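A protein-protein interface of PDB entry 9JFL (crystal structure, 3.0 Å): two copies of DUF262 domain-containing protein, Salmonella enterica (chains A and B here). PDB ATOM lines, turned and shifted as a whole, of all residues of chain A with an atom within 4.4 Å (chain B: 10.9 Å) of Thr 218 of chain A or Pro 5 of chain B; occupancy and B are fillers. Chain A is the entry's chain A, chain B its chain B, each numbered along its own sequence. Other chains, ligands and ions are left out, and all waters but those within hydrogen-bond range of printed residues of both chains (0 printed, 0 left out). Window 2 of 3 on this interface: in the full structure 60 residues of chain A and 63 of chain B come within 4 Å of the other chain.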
ATOM      1  N   VAL A  64      33.354  21.362 -30.862  1.00  0.00           N
ATOM      2  CA  VAL A  64      32.463  20.375 -30.287  1.00  0.00           C
ATOM      3  C   VAL A  64      32.371  19.167 -31.191  1.00  0.00           C
ATOM      4  O   VAL A  64      31.742  19.206 -32.259  1.00  0.00           O
ATOM      5  CB  VAL A  64      31.052  20.944 -30.098  1.00  0.00           C
ATOM      6  CG1 VAL A  64      30.143  19.922 -29.426  1.00  0.00           C
ATOM      7  CG2 VAL A  64      31.107  22.228 -29.284  1.00  0.00           C
ATOM      8  N   CYS A  65      32.999  18.085 -30.743  1.00  0.00           N
ATOM      9  CA  CYS A  65      32.990  16.822 -31.467  1.00  0.00           C
ATOM     10  C   CYS A  65      31.931  15.926 -30.876  1.00  0.00           C
ATOM     11  O   CYS A  65      31.494  16.148 -29.750  1.00  0.00           O
ATOM     12  CB  CYS A  65      34.353  16.146 -31.381  1.00  0.00           C
ATOM     13  SG  CYS A  65      35.715  17.268 -31.768  1.00  0.00           S
ATOM     14  N   ALA A  66      31.550  14.896 -31.629  1.00  0.00           N
ATOM     15  CA  ALA A  66      30.358  14.097 -31.325  1.00  0.00           C
ATOM     16  C   ALA A  66      30.662  12.674 -30.870  1.00  0.00           C
ATOM     17  O   ALA A  66      29.900  12.098 -30.088  1.00  0.00           O
ATOM     18  CB  ALA A  66      29.434  14.070 -32.530  1.00  0.00           C
ATOM     19  N   ILE A 216      35.317  20.219 -26.546  1.00  0.00           N
ATOM     20  CA  ILE A 216      34.233  19.586 -25.817  1.00  0.00           C
ATOM     21  C   ILE A 216      33.912  18.317 -26.554  1.00  0.00           C
ATOM     22  O   ILE A 216      33.714  18.339 -27.771  1.00  0.00           O
ATOM     23  CB  ILE A 216      32.953  20.446 -25.819  1.00  0.00           C
ATOM     24  CG1 ILE A 216      33.108  21.670 -24.922  1.00  0.00           C
ATOM     25  CG2 ILE A 216      31.750  19.642 -25.338  1.00  0.00           C
ATOM     26  CD1 ILE A 216      32.142  22.776 -25.289  1.00  0.00           C
ATOM     27  N   VAL A 217      33.836  17.211 -25.827  1.00  0.00           N
ATOM     28  CA  VAL A 217      33.434  15.958 -26.438  1.00  0.00           C
ATOM     29  C   VAL A 217      32.063  15.541 -25.941  1.00  0.00           C
ATOM     30  O   VAL A 217      31.864  15.286 -24.747  1.00  0.00           O
ATOM     31  CB  VAL A 217      34.434  14.835 -26.171  1.00  0.00           C
ATOM     32  CG1 VAL A 217      34.024  13.592 -26.951  1.00  0.00           C
ATOM     33  CG2 VAL A 217      35.834  15.290 -26.558  1.00  0.00           C
ATOM     34  N   THR A 218      31.127  15.459 -26.882  1.00  0.00           N
ATOM     35  CA  THR A 218      29.757  15.117 -26.564  1.00  0.00           C
ATOM     36  C   THR A 218      29.503  13.622 -26.784  1.00  0.00           C
ATOM     37  O   THR A 218      30.401  12.862 -27.148  1.00  0.00           O
ATOM     38  CB  THR A 218      28.766  15.978 -27.374  1.00  0.00           C
ATOM     39  OG1 THR A 218      28.970  15.760 -28.771  1.00  0.00           O
ATOM     40  CG2 THR A 218      28.964  17.445 -27.060  1.00  0.00           C
ATOM     41  N   ASN A 219      28.260  13.231 -26.545  1.00  0.00           N
ATOM     42  CA  ASN A 219      27.828  11.848 -26.468  1.00  0.00           C
ATOM     43  C   ASN A 219      27.129  11.416 -27.747  1.00  0.00           C
ATOM     44  O   ASN A 219      27.147  10.243 -28.099  1.00  0.00           O
ATOM     45  CB  ASN A 219      26.839  11.765 -25.303  1.00  0.00           C
ATOM     46  CG  ASN A 219      26.789  10.421 -24.624  1.00  0.00           C
ATOM     47  OD1 ASN A 219      26.427  10.354 -23.440  1.00  0.00           O
ATOM     48  ND2 ASN A 219      27.125   9.347 -25.343  1.00  0.00           N
ATOM     49  N   SER A 220      26.463  12.366 -28.398  1.00  0.00           N
ATOM     50  CA  SER A 220      25.724  12.120 -29.637  1.00  0.00           C
ATOM     51  C   SER A 220      25.623  13.425 -30.435  1.00  0.00           C
ATOM     52  O   SER A 220      25.885  14.499 -29.890  1.00  0.00           O
ATOM     53  CB  SER A 220      24.326  11.580 -29.319  1.00  0.00           C
ATOM     54  OG  SER A 220      23.474  12.590 -28.799  1.00  0.00           O
ATOM     55  N   ALA A 224      25.284  17.244 -29.060  1.00  0.00           N
ATOM     56  CA  ALA A 224      26.190  18.303 -29.505  1.00  0.00           C
ATOM     57  C   ALA A 224      25.380  19.491 -29.989  1.00  0.00           C
ATOM     58  O   ALA A 224      25.755  20.647 -29.769  1.00  0.00           O
ATOM     59  CB  ALA A 224      27.111  17.809 -30.613  1.00  0.00           C
ATOM     60  N   LEU A 227      23.593  21.718 -27.194  1.00  0.00           N
ATOM     61  CA  LEU A 227      24.461  22.779 -26.656  1.00  0.00           C
ATOM     62  C   LEU A 227      24.382  24.081 -27.447  1.00  0.00           C
ATOM     63  O   LEU A 227      24.947  25.088 -27.013  1.00  0.00           O
ATOM     64  CB  LEU A 227      25.926  22.332 -26.638  1.00  0.00           C
ATOM     65  CG  LEU A 227      26.450  21.486 -25.474  1.00  0.00           C
ATOM     66  CD1 LEU A 227      27.614  20.639 -25.951  1.00  0.00           C
ATOM     67  CD2 LEU A 227      26.880  22.366 -24.318  1.00  0.00           C
ATOM     68  N   LYS B   4      33.555   7.597 -24.400  1.00  0.00           N
ATOM     69  CA  LYS B   4      34.540   8.696 -24.138  1.00  0.00           C
ATOM     70  C   LYS B   4      34.038   9.737 -23.103  1.00  0.00           C
ATOM     71  O   LYS B   4      34.610   9.852 -22.012  1.00  0.00           O
ATOM     72  CB  LYS B   4      34.958   9.419 -25.445  1.00  0.00           C
ATOM     73  CG  LYS B   4      34.929   8.596 -26.729  1.00  0.00           C
ATOM     74  CD  LYS B   4      35.744   7.315 -26.633  1.00  0.00           C
ATOM     75  CE  LYS B   4      34.984   6.145 -27.237  1.00  0.00           C
ATOM     76  NZ  LYS B   4      35.732   4.866 -27.119  1.00  0.00           N
ATOM     77  N   PRO B   5      32.944  10.464 -23.427  1.00  0.00           N
ATOM     78  CA  PRO B   5      32.684  11.765 -22.798  1.00  0.00           C
ATOM     79  C   PRO B   5      32.297  11.699 -21.327  1.00  0.00           C
ATOM     80  O   PRO B   5      31.665  10.737 -20.901  1.00  0.00           O
ATOM     81  CB  PRO B   5      31.523  12.319 -23.627  1.00  0.00           C
ATOM     82  CG  PRO B   5      30.773  11.108 -24.056  1.00  0.00           C
ATOM     83  CD  PRO B   5      31.785  10.005 -24.219  1.00  0.00           C
ATOM     84  N   GLU B   6      32.673  12.737 -20.580  1.00  0.00           N
ATOM     85  CA  GLU B   6      32.357  12.856 -19.153  1.00  0.00           C
ATOM     86  C   GLU B   6      31.173  13.799 -19.004  1.00  0.00           C
ATOM     87  O   GLU B   6      31.203  14.925 -19.483  1.00  0.00           O
ATOM     88  CB  GLU B   6      33.571  13.367 -18.358  1.00  0.00           C
ATOM     89  CG  GLU B   6      33.295  13.714 -16.896  1.00  0.00           C
ATOM     90  CD  GLU B   6      33.062  15.202 -16.647  1.00  0.00           C
ATOM     91  OE1 GLU B   6      32.736  15.945 -17.593  1.00  0.00           O
ATOM     92  OE2 GLU B   6      33.211  15.644 -15.487  1.00  0.00           O
ATOM     93  N   TYR B   7      30.127  13.317 -18.349  1.00  0.00           N
ATOM     94  CA  TYR B   7      28.882  14.052 -18.180  1.00  0.00           C
ATOM     95  C   TYR B   7      28.566  14.070 -16.690  1.00  0.00           C
ATOM     96  O   TYR B   7      29.015  13.186 -15.955  1.00  0.00           O
ATOM     97  CB  TYR B   7      27.744  13.290 -18.854  1.00  0.00           C
ATOM     98  CG  TYR B   7      27.377  13.623 -20.284  1.00  0.00           C
ATOM     99  CD1 TYR B   7      28.313  14.033 -21.221  1.00  0.00           C
ATOM    100  CD2 TYR B   7      26.069  13.441 -20.709  1.00  0.00           C
ATOM    101  CE1 TYR B   7      27.937  14.277 -22.540  1.00  0.00           C
ATOM    102  CE2 TYR B   7      25.679  13.680 -22.007  1.00  0.00           C
ATOM    103  CZ  TYR B   7      26.602  14.102 -22.923  1.00  0.00           C
ATOM    104  OH  TYR B   7      26.147  14.331 -24.206  1.00  0.00           O
ATOM    105  N   MET B   8      27.766  15.031 -16.236  1.00  0.00           N
ATOM    106  CA  MET B   8      27.246  14.932 -14.876  1.00  0.00           C
ATOM    107  C   MET B   8      25.798  15.353 -14.658  1.00  0.00           C
ATOM    108  O   MET B   8      25.288  16.276 -15.275  1.00  0.00           O
ATOM    109  CB  MET B   8      28.153  15.649 -13.899  1.00  0.00           C
ATOM    110  CG  MET B   8      28.239  17.134 -14.071  1.00  0.00           C
ATOM    111  SD  MET B   8      29.520  17.687 -12.938  1.00  0.00           S
ATOM    112  CE  MET B   8      30.992  17.271 -13.885  1.00  0.00           C
ATOM    113  N   SER B   9      25.160  14.631 -13.747  1.00  0.00           N
ATOM    114  CA  SER B   9      23.791  14.859 -13.367  1.00  0.00           C
ATOM    115  C   SER B   9      23.632  16.132 -12.533  1.00  0.00           C
ATOM    116  O   SER B   9      24.597  16.667 -12.001  1.00  0.00           O
ATOM    117  CB  SER B   9      23.325  13.702 -12.506  1.00  0.00           C
ATOM    118  OG  SER B   9      23.782  13.918 -11.180  1.00  0.00           O
ATOM    119  N   GLU B  12      24.685  15.472  -8.885  1.00  0.00           N
ATOM    120  CA  GLU B  12      26.145  15.537  -8.772  1.00  0.00           C
ATOM    121  C   GLU B  12      26.627  17.000  -8.600  1.00  0.00           C
ATOM    122  O   GLU B  12      27.469  17.291  -7.743  1.00  0.00           O
ATOM    123  CB  GLU B  12      26.807  14.822  -9.960  1.00  0.00           C
ATOM    124  CG  GLU B  12      26.652  13.302  -9.874  1.00  0.00           C
ATOM    125  CD  GLU B  12      26.957  12.543 -11.169  1.00  0.00           C
ATOM    126  OE1 GLU B  12      27.387  13.166 -12.158  1.00  0.00           O
ATOM    127  OE2 GLU B  12      26.769  11.301 -11.192  1.00  0.00           O
ATOM    128  N   HIS B  58      19.404  14.573 -21.759  1.00  0.00           N
ATOM    129  CA  HIS B  58      20.543  15.491 -21.739  1.00  0.00           C
ATOM    130  C   HIS B  58      20.006  16.888 -21.605  1.00  0.00           C
ATOM    131  O   HIS B  58      20.111  17.720 -22.506  1.00  0.00           O
ATOM    132  CB  HIS B  58      21.390  15.372 -23.008  1.00  0.00           C
ATOM    133  CG  HIS B  58      22.550  16.324 -23.052  1.00  0.00           C
ATOM    134  ND1 HIS B  58      23.357  16.560 -21.962  1.00  0.00           N
ATOM    135  CD2 HIS B  58      23.036  17.094 -24.055  1.00  0.00           C
ATOM    136  CE1 HIS B  58      24.299  17.425 -22.293  1.00  0.00           C
ATOM    137  NE2 HIS B  58      24.125  17.769 -23.557  1.00  0.00           N
ATOM    138  N   PHE B  59      19.402  17.144 -20.463  1.00  0.00           N
ATOM    139  CA  PHE B  59      18.861  18.454 -20.205  1.00  0.00           C
ATOM    140  C   PHE B  59      19.915  19.476 -20.457  1.00  0.00           C
ATOM    141  O   PHE B  59      21.051  19.298 -20.051  1.00  0.00           O
ATOM    142  CB  PHE B  59      18.413  18.580 -18.772  1.00  0.00           C
ATOM    143  CG  PHE B  59      16.963  18.416 -18.604  1.00  0.00           C
ATOM    144  CD1 PHE B  59      16.114  19.410 -19.032  1.00  0.00           C
ATOM    145  CD2 PHE B  59      16.444  17.280 -18.027  1.00  0.00           C
ATOM    146  CE1 PHE B  59      14.754  19.288 -18.870  1.00  0.00           C
ATOM    147  CE2 PHE B  59      15.086  17.146 -17.864  1.00  0.00           C
ATOM    148  CZ  PHE B  59      14.243  18.153 -18.286  1.00  0.00           C
ATOM    149  N   PHE B  60      19.548  20.519 -21.182  1.00  0.00           N
ATOM    150  CA  PHE B  60      20.285  21.748 -21.130  1.00  0.00           C
ATOM    151  C   PHE B  60      21.774  21.453 -21.041  1.00  0.00           C
ATOM    152  O   PHE B  60      22.497  21.997 -20.193  1.00  0.00           O
ATOM    153  CB  PHE B  60      19.809  22.530 -19.902  1.00  0.00           C
ATOM    154  CG  PHE B  60      20.552  23.791 -19.677  1.00  0.00           C
ATOM    155  CD1 PHE B  60      20.515  24.792 -20.633  1.00  0.00           C
ATOM    156  CD2 PHE B  60      21.308  23.967 -18.542  1.00  0.00           C
ATOM    157  CE1 PHE B  60      21.220  25.958 -20.468  1.00  0.00           C
ATOM    158  CE2 PHE B  60      22.022  25.130 -18.367  1.00  0.00           C
ATOM    159  CZ  PHE B  60      21.976  26.131 -19.333  1.00  0.00           C
ATOM    160  N   GLY B  61      22.241  20.563 -21.901  1.00  0.00           N
ATOM    161  CA  GLY B  61      23.643  20.234 -21.874  1.00  0.00           C
ATOM    162  C   GLY B  61      24.396  21.526 -21.784  1.00  0.00           C
ATOM    163  O   GLY B  61      24.255  22.381 -22.658  1.00  0.00           O
ATOM    164  N   GLY B  62      25.138  21.709 -20.707  1.00  0.00           N
ATOM    165  CA  GLY B  62      26.004  22.864 -20.621  1.00  0.00           C
ATOM    166  C   GLY B  62      25.596  23.800 -19.522  1.00  0.00           C
ATOM    167  O   GLY B  62      24.713  24.624 -19.704  1.00  0.00           O
ATOM    168  N   LEU B 212      21.137  14.807 -17.045  1.00  0.00           N
ATOM    169  CA  LEU B 212      22.552  15.153 -17.171  1.00  0.00           C
ATOM    170  C   LEU B 212      22.796  16.551 -17.758  1.00  0.00           C
ATOM    171  O   LEU B 212      21.908  17.152 -18.349  1.00  0.00           O
ATOM    172  CB  LEU B 212      23.226  14.116 -18.075  1.00  0.00           C
ATOM    173  CG  LEU B 212      22.914  12.634 -17.815  1.00  0.00           C
ATOM    174  CD1 LEU B 212      23.673  11.742 -18.780  1.00  0.00           C
ATOM    175  CD2 LEU B 212      23.258  12.257 -16.385  1.00  0.00           C
ATOM    176  N   VAL B 213      24.015  17.060 -17.586  1.00  0.00           N
ATOM    177  CA  VAL B 213      24.494  18.267 -18.292  1.00  0.00           C
ATOM    178  C   VAL B 213      25.983  18.106 -18.517  1.00  0.00           C
ATOM    179  O   VAL B 213      26.622  17.290 -17.847  1.00  0.00           O
ATOM    180  CB  VAL B 213      24.317  19.595 -17.496  1.00  0.00           C
ATOM    181  CG1 VAL B 213      22.865  19.988 -17.364  1.00  0.00           C
ATOM    182  CG2 VAL B 213      24.976  19.506 -16.124  1.00  0.00           C
ATOM    183  N   ILE B 214      26.534  18.893 -19.436  1.00  0.00           N
ATOM    184  CA  ILE B 214      27.980  19.049 -19.521  1.00  0.00           C
ATOM    185  C   ILE B 214      28.406  20.250 -18.672  1.00  0.00           C
ATOM    186  O   ILE B 214      28.091  21.385 -18.991  1.00  0.00           O
ATOM    187  CB  ILE B 214      28.440  19.207 -20.981  1.00  0.00           C
ATOM    188  CG1 ILE B 214      28.155  17.923 -21.757  1.00  0.00           C
ATOM    189  CG2 ILE B 214      29.929  19.487 -21.050  1.00  0.00           C
ATOM    190  CD1 ILE B 214      28.162  18.084 -23.264  1.00  0.00           C
ATOM    191  N   HIS B 215      29.120  19.994 -17.584  1.00  0.00           N
ATOM    192  CA  HIS B 215      29.675  21.077 -16.765  1.00  0.00           C
ATOM    193  C   HIS B 215      30.929  21.592 -17.428  1.00  0.00           C
ATOM    194  O   HIS B 215      31.912  20.866 -17.558  1.00  0.00           O
ATOM    195  CB  HIS B 215      30.016  20.573 -15.372  1.00  0.00           C
ATOM    196  CG  HIS B 215      30.456  21.647 -14.433  1.00  0.00           C
ATOM    197  ND1 HIS B 215      31.743  21.729 -13.948  1.00  0.00           N
ATOM    198  CD2 HIS B 215      29.775  22.674 -13.871  1.00  0.00           C
ATOM    199  CE1 HIS B 215      31.837  22.763 -13.130  1.00  0.00           C
ATOM    200  NE2 HIS B 215      30.657  23.352 -13.063  1.00  0.00           N
ATOM    201  N   ILE B 216      30.891  22.839 -17.867  1.00  0.00           N
ATOM    202  CA  ILE B 216      32.015  23.413 -18.580  1.00  0.00           C
ATOM    203  C   ILE B 216      32.562  24.508 -17.728  1.00  0.00           C
ATOM    204  O   ILE B 216      31.830  25.385 -17.293  1.00  0.00           O
ATOM    205  CB  ILE B 216      31.599  24.009 -19.924  1.00  0.00           C
ATOM    206  CG1 ILE B 216      30.937  22.929 -20.779  1.00  0.00           C
ATOM    207  CG2 ILE B 216      32.812  24.606 -20.619  1.00  0.00           C
ATOM    208  CD1 ILE B 216      30.553  23.394 -22.163  1.00  0.00           C
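Ile 216 of chain B touches its own counterpart, Ile 216 of chain A.
1 position is printed for both chains.
Of the 9 pairs that touch across the chains among the printed residues, 1 has its exchanged pair printed and touching as well.
Among the printed residues, merely in contact across the chains: Ile 216 of chain A with Ile 216 of chain B (3.6 Å), Val 217 of chain A with Pro 5 of chain B (3.2 Å), Thr 218 of chain A with Pro 5 of chain B (3.6 Å), Thr 218 of chain A with Ile 214 of chain B (3.9 Å), Asn 219 of chain A with Pro 5 of chain B (3.9 Å), Leu 227 of chain A with Gly 61 of chain B (3.1 Å), Leu 227 of chain A with Gly 62 of chain B (3.8 Å) and Leu 227 of chain A with Ile 214 of chain B (3.7 Å).
O of Cys 65 of chain A is in hydrogen-bond range of OG1 of Thr 218 of chain A, 2.7 Å away.
The backbone NH (N) of Gly 62 of chain B lies close to the backbone carbonyl oxygen (O) of Ile 214 of chain B.
O of Ile 216 of chain A sits at hydrogen-bond distance from N of Cys 65 of chain A (3.1 Å).
Thr 218 of chain A touches just these residues of chain B: Pro 5 and Ile 214.
Pro 5 of chain B touches three residues of chain A.
Of chain B, only Pro 5 (3.9 Å) and Tyr 7 (2.9 Å) come within 4 Å of Asn 219 of chain A.
Of the printed residues of chain A, Gly 61 of chain B touches Leu 227 (3.1 Å).
Printed residues of chain B within 4 Å of Leu 227 of chain A: Gly 61 (3.1 Å), Gly 62 (3.8 Å) and Ile 214 (3.7 Å).
Printed residues of chain A within 4 Å of Ile 216 of chain B: Ile 216 (3.6 Å).
His 215 of chain B touches none of the printed residues of chain A.
The nearest residue of chain B that does not touch Thr 218 of chain A is Tyr 7 of chain B (4.3 Å).
The nearest printed residue of chain A that does not touch Pro 5 of chain B is Ala 66 of chain A (6.2 Å).
The nearest printed residue of chain A that does not touch Gly 61 of chain B is Ala 224 of chain A (7.5 Å).
Of the 10 printed residues of chain A, 5 touch a printed residue of chain B.
Printed residues of chain B that touch a printed residue of chain A: Pro 5, Tyr 7, Gly 61, Gly 62, Ile 214 and Ile 216.
Hydrophobic or aromatic side chains of chain B that line the printed part of chain A: Pro 5, Tyr 7, Ile 214 and Ile 216.
Along chain B the printed residues that touch a printed residue of chain A span positions 5 to 216.
Among the printed residues, no Asp or Glu carboxylate lies within 4 Å of a Lys or Arg side-chain nitrogen of the other chain.
N of Asn 219 of chain A lies close to OH of Tyr 7 of chain B, at 3.3 Å.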
